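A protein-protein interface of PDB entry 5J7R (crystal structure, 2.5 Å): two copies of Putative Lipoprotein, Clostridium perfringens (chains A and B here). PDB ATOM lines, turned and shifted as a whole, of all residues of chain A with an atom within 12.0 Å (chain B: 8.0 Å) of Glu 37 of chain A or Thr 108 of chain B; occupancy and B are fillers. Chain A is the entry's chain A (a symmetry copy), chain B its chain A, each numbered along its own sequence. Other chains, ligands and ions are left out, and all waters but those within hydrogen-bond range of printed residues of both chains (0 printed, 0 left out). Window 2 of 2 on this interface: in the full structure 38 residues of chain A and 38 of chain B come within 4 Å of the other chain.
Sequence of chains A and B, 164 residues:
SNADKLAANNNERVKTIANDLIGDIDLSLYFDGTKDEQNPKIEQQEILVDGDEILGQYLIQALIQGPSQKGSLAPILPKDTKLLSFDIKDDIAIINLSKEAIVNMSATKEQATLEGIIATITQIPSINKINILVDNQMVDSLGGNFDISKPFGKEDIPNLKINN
Hydrophobic or aromatic side chains of chain B that line the printed part of chain A: Ala 112. Of the 14 printed residues of chain A, 4 touch a printed residue of chain B. Printed residues of chain A that touch a printed residue of chain B: Asp 32, Glu 37, Pro 40 and Ile 42. Among the printed residues, 7 pairs touch across the chains. Among the printed residues, Asp or Glu carboxylates within 4 Å of a Lys or Arg side-chain nitrogen of the other chain: Asp 32 of chain A with Lys 109 of chain B (3.0 Å).
Glu 37 of chain A touches just one residue of chain B: Thr 108. Of the printed residues of chain A, Thr 108 of chain B touches Glu 37 (2.8 Å) and Pro 40 (3.3 Å). No residue of chain A comes within 4 Å of Ala 107 of chain B. Of chain A, only Asp 32 (3.0 Å) comes within 4 Å of Lys 109 of chain B. Printed residues of chain B within 4 Å of Pro 40 of chain A: Thr 108 and Gln 111. Printed residues of chain B within 4 Å of Ile 42 of chain A: Ala 112 (3.5 Å) and Glu 115 (3.6 Å). Of the printed residues of chain B, Asp 32 of chain A touches Lys 109 (3.0 Å) and Ala 112 (3.7 Å). Tyr 30 of chain A touches none of the printed residues of chain B. The nearest residue of chain B that does not touch Glu 37 of chain A is Ser 106 of chain B (5.1 Å). The nearest residue of chain A that does not touch Thr 108 of chain B is Gln 38 of chain A (4.4 Å). The nearest printed residue of chain A that does not touch Glu 115 of chain B is Pro 40 of chain A (4.1 Å).
Ala 112 of chain B touches Asp 32 of chain A. Thr 108 of chain B touches Glu 37 of chain A. CB of Pro 40 of chain A touches O of Thr 108 of chain B, 3.3 Å away. CG of Pro 40 of chain A touches CD of Gln 111 of chain B, 3.4 Å away. Ile 42 of chain A touches Ala 112 of chain B (CG2 to O, 3.5 Å). CD1 of Ile 42 of chain A touches O of Glu 115 of chain B (3.6 Å).
No position is printed for both chains. Of the 7 pairs that touch across the chains among the printed residues, none has its exchanged pair printed and touching as well.
NZ of Lys 109 of chain B is in salt-bridge range of OD2 of Asp 32 of chain A (3.0 Å).
The backbone carbonyl oxygen (O) of Lys 109 of chain B sits at hydrogen-bond distance from the side-chain hydroxyl (OG1) of Thr 113 of chain B (3.3 Å). The side-chain carboxylate (OD1) of Asp 32 of chain A sits at hydrogen-bond distance from the side-chain hydroxyl (OG1) of Thr 34 of chain A. NE2 of Gln 111 of chain B is in hydrogen-bond range of OE2 of Glu 115 of chain B. The side-chain hydroxyl (OG) of Ser 106 of chain B lies within hydrogen-bond range of the side-chain hydroxyl (OG1) of Thr 108 of chain B. N of Lys 109 of chain B lies within hydrogen-bond range of OG of Ser 106 of chain B, 3.2 Å away.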
ATOM      1  N   TYR A  30     -14.454  11.861  -5.010  1.00  0.00           N
ATOM      2  CA  TYR A  30     -14.674  11.305  -6.332  1.00  0.00           C
ATOM      3  C   TYR A  30     -14.482  12.351  -7.395  1.00  0.00           C
ATOM      4  O   TYR A  30     -15.243  13.310  -7.468  1.00  0.00           O
ATOM      5  CB  TYR A  30     -16.071  10.713  -6.440  1.00  0.00           C
ATOM      6  CG  TYR A  30     -16.266   9.506  -5.577  1.00  0.00           C
ATOM      7  CD1 TYR A  30     -16.648   9.635  -4.265  1.00  0.00           C
ATOM      8  CD2 TYR A  30     -16.071   8.217  -6.086  1.00  0.00           C
ATOM      9  CE1 TYR A  30     -16.833   8.530  -3.462  1.00  0.00           C
ATOM     10  CE2 TYR A  30     -16.263   7.096  -5.293  1.00  0.00           C
ATOM     11  CZ  TYR A  30     -16.647   7.262  -3.977  1.00  0.00           C
ATOM     12  OH  TYR A  30     -16.832   6.182  -3.155  1.00  0.00           O
ATOM     13  N   PHE A  31     -13.445  12.163  -8.205  1.00  0.00           N
ATOM     14  CA  PHE A  31     -13.130  13.067  -9.306  1.00  0.00           C
ATOM     15  C   PHE A  31     -13.416  12.400 -10.644  1.00  0.00           C
ATOM     16  O   PHE A  31     -13.842  11.244 -10.695  1.00  0.00           O
ATOM     17  CB  PHE A  31     -11.682  13.539  -9.223  1.00  0.00           C
ATOM     18  CG  PHE A  31     -11.420  14.427  -8.053  1.00  0.00           C
ATOM     19  CD1 PHE A  31     -11.797  15.766  -8.092  1.00  0.00           C
ATOM     20  CD2 PHE A  31     -10.781  13.946  -6.918  1.00  0.00           C
ATOM     21  CE1 PHE A  31     -11.560  16.596  -7.011  1.00  0.00           C
ATOM     22  CE2 PHE A  31     -10.533  14.776  -5.842  1.00  0.00           C
ATOM     23  CZ  PHE A  31     -10.921  16.100  -5.888  1.00  0.00           C
ATOM     24  N   ASP A  32     -13.196  13.143 -11.722  1.00  0.00           N
ATOM     25  CA  ASP A  32     -13.449  12.638 -13.067  1.00  0.00           C
ATOM     26  C   ASP A  32     -12.317  11.711 -13.537  1.00  0.00           C
ATOM     27  O   ASP A  32     -11.168  12.141 -13.690  1.00  0.00           O
ATOM     28  CB  ASP A  32     -13.607  13.826 -14.030  1.00  0.00           C
ATOM     29  CG  ASP A  32     -14.036  13.414 -15.424  1.00  0.00           C
ATOM     30  OD1 ASP A  32     -14.374  12.237 -15.644  1.00  0.00           O
ATOM     31  OD2 ASP A  32     -14.057  14.288 -16.314  1.00  0.00           O
ATOM     32  N   GLY A  33     -12.649  10.440 -13.747  1.00  0.00           N
ATOM     33  CA  GLY A  33     -11.687   9.434 -14.229  1.00  0.00           C
ATOM     34  C   GLY A  33     -12.048   8.924 -15.623  1.00  0.00           C
ATOM     35  O   GLY A  33     -11.688   7.802 -15.987  1.00  0.00           O
ATOM     36  N   THR A  34     -12.730   9.763 -16.408  1.00  0.00           N
ATOM     37  CA  THR A  34     -13.183   9.396 -17.757  1.00  0.00           C
ATOM     38  C   THR A  34     -12.094   9.353 -18.851  1.00  0.00           C
ATOM     39  O   THR A  34     -11.186  10.204 -18.956  1.00  0.00           O
ATOM     40  CB  THR A  34     -14.402  10.282 -18.190  1.00  0.00           C
ATOM     41  OG1 THR A  34     -15.500  10.113 -17.274  1.00  0.00           O
ATOM     42  CG2 THR A  34     -14.881   9.923 -19.591  1.00  0.00           C
ATOM     43  N   LYS A  35     -12.222   8.318 -19.672  1.00  0.00           N
ATOM     44  CA  LYS A  35     -11.325   8.094 -20.805  1.00  0.00           C
ATOM     45  C   LYS A  35     -12.201   7.984 -22.051  1.00  0.00           C
ATOM     46  O   LYS A  35     -12.025   8.729 -23.020  1.00  0.00           O
ATOM     47  CB  LYS A  35     -10.483   6.829 -20.577  1.00  0.00           C
ATOM     48  CG  LYS A  35      -9.754   6.820 -19.189  1.00  0.00           C
ATOM     49  CD  LYS A  35      -8.831   5.565 -18.955  1.00  0.00           C
ATOM     50  CE  LYS A  35      -7.374   5.920 -19.250  1.00  0.00           C
ATOM     51  NZ  LYS A  35      -6.491   4.731 -19.409  1.00  0.00           N
ATOM     52  N   ASP A  36     -13.165   7.067 -21.995  1.00  0.00           N
ATOM     53  CA  ASP A  36     -14.116   6.838 -23.075  1.00  0.00           C
ATOM     54  C   ASP A  36     -15.244   7.850 -23.002  1.00  0.00           C
ATOM     55  O   ASP A  36     -16.074   7.765 -22.097  1.00  0.00           O
ATOM     56  CB  ASP A  36     -14.706   5.406 -23.014  1.00  0.00           C
ATOM     57  CG  ASP A  36     -13.678   4.304 -23.308  1.00  0.00           C
ATOM     58  OD1 ASP A  36     -12.488   4.604 -23.569  1.00  0.00           O
ATOM     59  OD2 ASP A  36     -14.078   3.113 -23.291  1.00  0.00           O
ATOM     60  N   GLU A  37     -15.259   8.801 -23.952  1.00  0.00           N
ATOM     61  CA  GLU A  37     -16.328   9.815 -24.021  1.00  0.00           C
ATOM     62  C   GLU A  37     -17.767   9.226 -24.058  1.00  0.00           C
ATOM     63  O   GLU A  37     -18.727   9.956 -24.017  1.00  0.00           O
ATOM     64  CB  GLU A  37     -16.112  10.838 -25.167  1.00  0.00           C
ATOM     65  CG  GLU A  37     -17.264  11.813 -25.418  1.00  0.00           C
ATOM     66  CD  GLU A  37     -16.951  12.855 -26.481  1.00  0.00           C
ATOM     67  OE1 GLU A  37     -17.727  13.827 -26.617  1.00  0.00           O
ATOM     68  OE2 GLU A  37     -15.926  12.716 -27.176  1.00  0.00           O
ATOM     69  N   GLN A  38     -17.898   7.910 -24.161  1.00  0.00           N
ATOM     70  CA  GLN A  38     -19.192   7.240 -24.177  1.00  0.00           C
ATOM     71  C   GLN A  38     -19.707   7.016 -22.751  1.00  0.00           C
ATOM     72  O   GLN A  38     -20.895   7.218 -22.478  1.00  0.00           O
ATOM     73  CB  GLN A  38     -19.044   5.897 -24.932  1.00  0.00           C
ATOM     74  CG  GLN A  38     -20.243   4.949 -24.855  1.00  0.00           C
ATOM     75  CD  GLN A  38     -21.547   5.485 -25.419  1.00  0.00           C
ATOM     76  OE1 GLN A  38     -21.569   6.373 -26.272  1.00  0.00           O
ATOM     77  NE2 GLN A  38     -22.655   4.906 -24.961  1.00  0.00           N
ATOM     78  N   ASN A  39     -18.807   6.628 -21.849  1.00  0.00           N
ATOM     79  CA  ASN A  39     -19.145   6.336 -20.462  1.00  0.00           C
ATOM     80  C   ASN A  39     -18.491   7.229 -19.405  1.00  0.00           C
ATOM     81  O   ASN A  39     -17.289   7.094 -19.151  1.00  0.00           O
ATOM     82  CB  ASN A  39     -18.745   4.888 -20.186  1.00  0.00           C
ATOM     83  CG  ASN A  39     -19.723   3.897 -20.772  1.00  0.00           C
ATOM     84  OD1 ASN A  39     -20.703   4.278 -21.412  1.00  0.00           O
ATOM     85  ND2 ASN A  39     -19.476   2.619 -20.536  1.00  0.00           N
ATOM     86  N   PRO A  40     -19.284   8.118 -18.763  1.00  0.00           N
ATOM     87  CA  PRO A  40     -18.711   8.970 -17.721  1.00  0.00           C
ATOM     88  C   PRO A  40     -18.363   8.106 -16.516  1.00  0.00           C
ATOM     89  O   PRO A  40     -19.174   7.282 -16.074  1.00  0.00           O
ATOM     90  CB  PRO A  40     -19.827   9.969 -17.416  1.00  0.00           C
ATOM     91  CG  PRO A  40     -21.082   9.260 -17.763  1.00  0.00           C
ATOM     92  CD  PRO A  40     -20.746   8.290 -18.867  1.00  0.00           C
ATOM     93  N   LYS A  41     -17.157   8.297 -15.999  1.00  0.00           N
ATOM     94  CA  LYS A  41     -16.666   7.512 -14.888  1.00  0.00           C
ATOM     95  C   LYS A  41     -15.971   8.348 -13.815  1.00  0.00           C
ATOM     96  O   LYS A  41     -15.251   9.288 -14.124  1.00  0.00           O
ATOM     97  CB  LYS A  41     -15.727   6.459 -15.465  1.00  0.00           C
ATOM     98  CG  LYS A  41     -15.051   5.584 -14.434  1.00  0.00           C
ATOM     99  CD  LYS A  41     -14.529   4.250 -15.053  1.00  0.00           C
ATOM    100  CE  LYS A  41     -15.615   3.161 -15.048  1.00  0.00           C
ATOM    101  NZ  LYS A  41     -15.216   1.882 -15.705  1.00  0.00           N
ATOM    102  N   ILE A  42     -16.196   7.982 -12.556  1.00  0.00           N
ATOM    103  CA  ILE A  42     -15.593   8.677 -11.418  1.00  0.00           C
ATOM    104  C   ILE A  42     -14.682   7.713 -10.651  1.00  0.00           C
ATOM    105  O   ILE A  42     -15.009   6.542 -10.494  1.00  0.00           O
ATOM    106  CB  ILE A  42     -16.664   9.304 -10.490  1.00  0.00           C
ATOM    107  CG1 ILE A  42     -17.647   8.244  -9.973  1.00  0.00           C
ATOM    108  CG2 ILE A  42     -17.431  10.393 -11.235  1.00  0.00           C
ATOM    109  CD1 ILE A  42     -18.723   8.781  -9.043  1.00  0.00           C
ATOM    110  N   GLU A  43     -13.528   8.210 -10.218  1.00  0.00           N
ATOM    111  CA  GLU A  43     -12.549   7.425  -9.454  1.00  0.00           C
ATOM    112  C   GLU A  43     -12.268   8.111  -8.104  1.00  0.00           C
ATOM    113  O   GLU A  43     -12.299   9.330  -7.991  1.00  0.00           O
ATOM    114  CB  GLU A  43     -11.276   7.168 -10.291  1.00  0.00           C
ATOM    115  CG  GLU A  43     -11.347   5.916 -11.139  1.00  0.00           C
ATOM    116  CD  GLU A  43     -10.201   5.809 -12.118  1.00  0.00           C
ATOM    117  OE1 GLU A  43     -10.413   5.337 -13.262  1.00  0.00           O
ATOM    118  OE2 GLU A  43      -9.093   6.243 -11.752  1.00  0.00           O
ATOM    119  N   MET B 105     -20.216  22.655 -20.687  1.00  0.00           N
ATOM    120  CA  MET B 105     -19.666  21.305 -20.524  1.00  0.00           C
ATOM    121  C   MET B 105     -20.340  20.301 -21.419  1.00  0.00           C
ATOM    122  O   MET B 105     -21.494  20.478 -21.813  1.00  0.00           O
ATOM    123  CB  MET B 105     -19.908  20.752 -19.114  1.00  0.00           C
ATOM    124  CG  MET B 105     -19.352  21.578 -17.953  1.00  0.00           C
ATOM    125  SD  MET B 105     -19.851  20.699 -16.243  1.00  0.00           S
ATOM    126  CE  MET B 105     -19.674  22.262 -15.057  1.00  0.00           C
ATOM    127  N   SER B 106     -19.615  19.225 -21.729  1.00  0.00           N
ATOM    128  CA  SER B 106     -20.154  18.136 -22.541  1.00  0.00           C
ATOM    129  C   SER B 106     -21.042  17.323 -21.613  1.00  0.00           C
ATOM    130  O   SER B 106     -20.855  17.349 -20.388  1.00  0.00           O
ATOM    131  CB  SER B 106     -19.041  17.248 -23.086  1.00  0.00           C
ATOM    132  OG  SER B 106     -18.298  16.652 -22.034  1.00  0.00           O
ATOM    133  N   ALA B 107     -22.006  16.608 -22.176  1.00  0.00           N
ATOM    134  CA  ALA B 107     -22.909  15.799 -21.358  1.00  0.00           C
ATOM    135  C   ALA B 107     -22.190  14.717 -20.547  1.00  0.00           C
ATOM    136  O   ALA B 107     -22.637  14.368 -19.452  1.00  0.00           O
ATOM    137  CB  ALA B 107     -23.981  15.184 -22.220  1.00  0.00           C
ATOM    138  N   THR B 108     -21.082  14.202 -21.070  1.00  0.00           N
ATOM    139  CA  THR B 108     -20.322  13.170 -20.358  1.00  0.00           C
ATOM    140  C   THR B 108     -19.548  13.789 -19.188  1.00  0.00           C
ATOM    141  O   THR B 108     -19.477  13.188 -18.119  1.00  0.00           O
ATOM    142  CB  THR B 108     -19.404  12.337 -21.290  1.00  0.00           C
ATOM    143  OG1 THR B 108     -18.497  13.210 -21.971  1.00  0.00           O
ATOM    144  CG2 THR B 108     -20.257  11.575 -22.305  1.00  0.00           C
ATOM    145  N   LYS B 109     -18.999  14.990 -19.378  1.00  0.00           N
ATOM    146  CA  LYS B 109     -18.246  15.674 -18.319  1.00  0.00           C
ATOM    147  C   LYS B 109     -19.206  16.148 -17.222  1.00  0.00           C
ATOM    148  O   LYS B 109     -18.936  15.963 -16.028  1.00  0.00           O
ATOM    149  CB  LYS B 109     -17.460  16.859 -18.899  1.00  0.00           C
ATOM    150  CG  LYS B 109     -16.575  17.632 -17.960  1.00  0.00           C
ATOM    151  CD  LYS B 109     -15.323  16.860 -17.576  1.00  0.00           C
ATOM    152  CE  LYS B 109     -14.603  17.545 -16.380  1.00  0.00           C
ATOM    153  NZ  LYS B 109     -13.192  17.129 -16.112  1.00  0.00           N
ATOM    154  N   GLU B 110     -20.332  16.735 -17.626  1.00  0.00           N
ATOM    155  CA  GLU B 110     -21.322  17.227 -16.668  1.00  0.00           C
ATOM    156  C   GLU B 110     -21.901  16.081 -15.844  1.00  0.00           C
ATOM    157  O   GLU B 110     -22.157  16.247 -14.653  1.00  0.00           O
ATOM    158  CB  GLU B 110     -22.450  18.002 -17.357  1.00  0.00           C
ATOM    159  CG  GLU B 110     -23.468  18.584 -16.371  1.00  0.00           C
ATOM    160  CD  GLU B 110     -24.564  19.417 -17.014  1.00  0.00           C
ATOM    161  OE1 GLU B 110     -24.858  19.170 -18.187  1.00  0.00           O
ATOM    162  OE2 GLU B 110     -25.155  20.296 -16.332  1.00  0.00           O
ATOM    163  N   GLN B 111     -22.104  14.926 -16.467  1.00  0.00           N
ATOM    164  CA  GLN B 111     -22.649  13.782 -15.738  1.00  0.00           C
ATOM    165  C   GLN B 111     -21.646  13.287 -14.691  1.00  0.00           C
ATOM    166  O   GLN B 111     -22.043  12.861 -13.611  1.00  0.00           O
ATOM    167  CB  GLN B 111     -23.050  12.650 -16.683  1.00  0.00           C
ATOM    168  CG  GLN B 111     -23.679  11.472 -15.956  1.00  0.00           C
ATOM    169  CD  GLN B 111     -24.197  10.391 -16.879  1.00  0.00           C
ATOM    170  OE1 GLN B 111     -24.332  10.591 -18.086  1.00  0.00           O
ATOM    171  NE2 GLN B 111     -24.507   9.234 -16.306  1.00  0.00           N
ATOM    172  N   ALA B 112     -20.357  13.349 -15.013  1.00  0.00           N
ATOM    173  CA  ALA B 112     -19.309  12.916 -14.082  1.00  0.00           C
ATOM    174  C   ALA B 112     -19.262  13.870 -12.893  1.00  0.00           C
ATOM    175  O   ALA B 112     -19.067  13.448 -11.757  1.00  0.00           O
ATOM    176  CB  ALA B 112     -17.961  12.861 -14.777  1.00  0.00           C
ATOM    177  N   THR B 113     -19.453  15.159 -13.163  1.00  0.00           N
ATOM    178  CA  THR B 113     -19.465  16.175 -12.123  1.00  0.00           C
ATOM    179  C   THR B 113     -20.578  15.915 -11.120  1.00  0.00           C
ATOM    180  O   THR B 113     -20.329  15.863  -9.916  1.00  0.00           O
ATOM    181  CB  THR B 113     -19.641  17.581 -12.718  1.00  0.00           C
ATOM    182  OG1 THR B 113     -18.472  17.924 -13.467  1.00  0.00           O
ATOM    183  CG2 THR B 113     -19.848  18.629 -11.619  1.00  0.00           C
ATOM    184  N   LEU B 114     -21.799  15.735 -11.610  1.00  0.00           N
ATOM    185  CA  LEU B 114     -22.939  15.483 -10.724  1.00  0.00           C
ATOM    186  C   LEU B 114     -22.784  14.156  -9.964  1.00  0.00           C
ATOM    187  O   LEU B 114     -23.092  14.085  -8.771  1.00  0.00           O
ATOM    188  CB  LEU B 114     -24.258  15.537 -11.500  1.00  0.00           C
ATOM    189  CG  LEU B 114     -24.505  16.837 -12.290  1.00  0.00           C
ATOM    190  CD1 LEU B 114     -25.863  16.769 -12.978  1.00  0.00           C
ATOM    191  CD2 LEU B 114     -24.411  18.093 -11.434  1.00  0.00           C
ATOM    192  N   GLU B 115     -22.297  13.118 -10.640  1.00  0.00           N
ATOM    193  CA  GLU B 115     -22.088  11.825  -9.984  1.00  0.00           C
ATOM    194  C   GLU B 115     -20.961  11.919  -8.944  1.00  0.00           C
ATOM    195  O   GLU B 115     -21.027  11.264  -7.906  1.00  0.00           O
ATOM    196  CB  GLU B 115     -21.789  10.714 -10.995  1.00  0.00           C
ATOM    197  CG  GLU B 115     -22.977  10.341 -11.872  1.00  0.00           C
ATOM    198  CD  GLU B 115     -22.681   9.232 -12.878  1.00  0.00           C
ATOM    199  OE1 GLU B 115     -21.500   8.902 -13.059  1.00  0.00           O
ATOM    200  OE2 GLU B 115     -23.627   8.700 -13.508  1.00  0.00           O
ATOM    201  N   ASN B 145     -26.476  20.326 -20.021  1.00  0.00           N
ATOM    202  CA  ASN B 145     -27.105  19.026 -20.352  1.00  0.00           C
ATOM    203  C   ASN B 145     -27.936  18.333 -19.266  1.00  0.00           C
ATOM    204  O   ASN B 145     -28.538  17.295 -19.528  1.00  0.00           O
ATOM    205  CB  ASN B 145     -26.027  18.036 -20.796  1.00  0.00           C
ATOM    206  CG  ASN B 145     -25.083  18.615 -21.852  1.00  0.00           C
ATOM    207  OD1 ASN B 145     -25.490  18.779 -22.990  1.00  0.00           O
ATOM    208  ND2 ASN B 145     -23.805  18.857 -21.505  1.00  0.00           N
ATOM    209  N   PHE B 146     -27.948  18.868 -18.053  1.00  0.00           N
ATOM    210  CA  PHE B 146     -28.693  18.261 -16.953  1.00  0.00           C
ATOM    211  C   PHE B 146     -29.506  19.267 -16.165  1.00  0.00           C
ATOM    212  O   PHE B 146     -29.037  20.358 -15.852  1.00  0.00           O
ATOM    213  CB  PHE B 146     -27.758  17.474 -16.029  1.00  0.00           C
ATOM    214  CG  PHE B 146     -27.270  16.191 -16.624  1.00  0.00           C
ATOM    215  CD1 PHE B 146     -26.133  16.161 -17.414  1.00  0.00           C
ATOM    216  CD2 PHE B 146     -27.963  15.002 -16.402  1.00  0.00           C
ATOM    217  CE1 PHE B 146     -25.690  14.975 -17.971  1.00  0.00           C
ATOM    218  CE2 PHE B 146     -27.525  13.814 -16.955  1.00  0.00           C
ATOM    219  CZ  PHE B 146     -26.386  13.800 -17.744  1.00  0.00           C
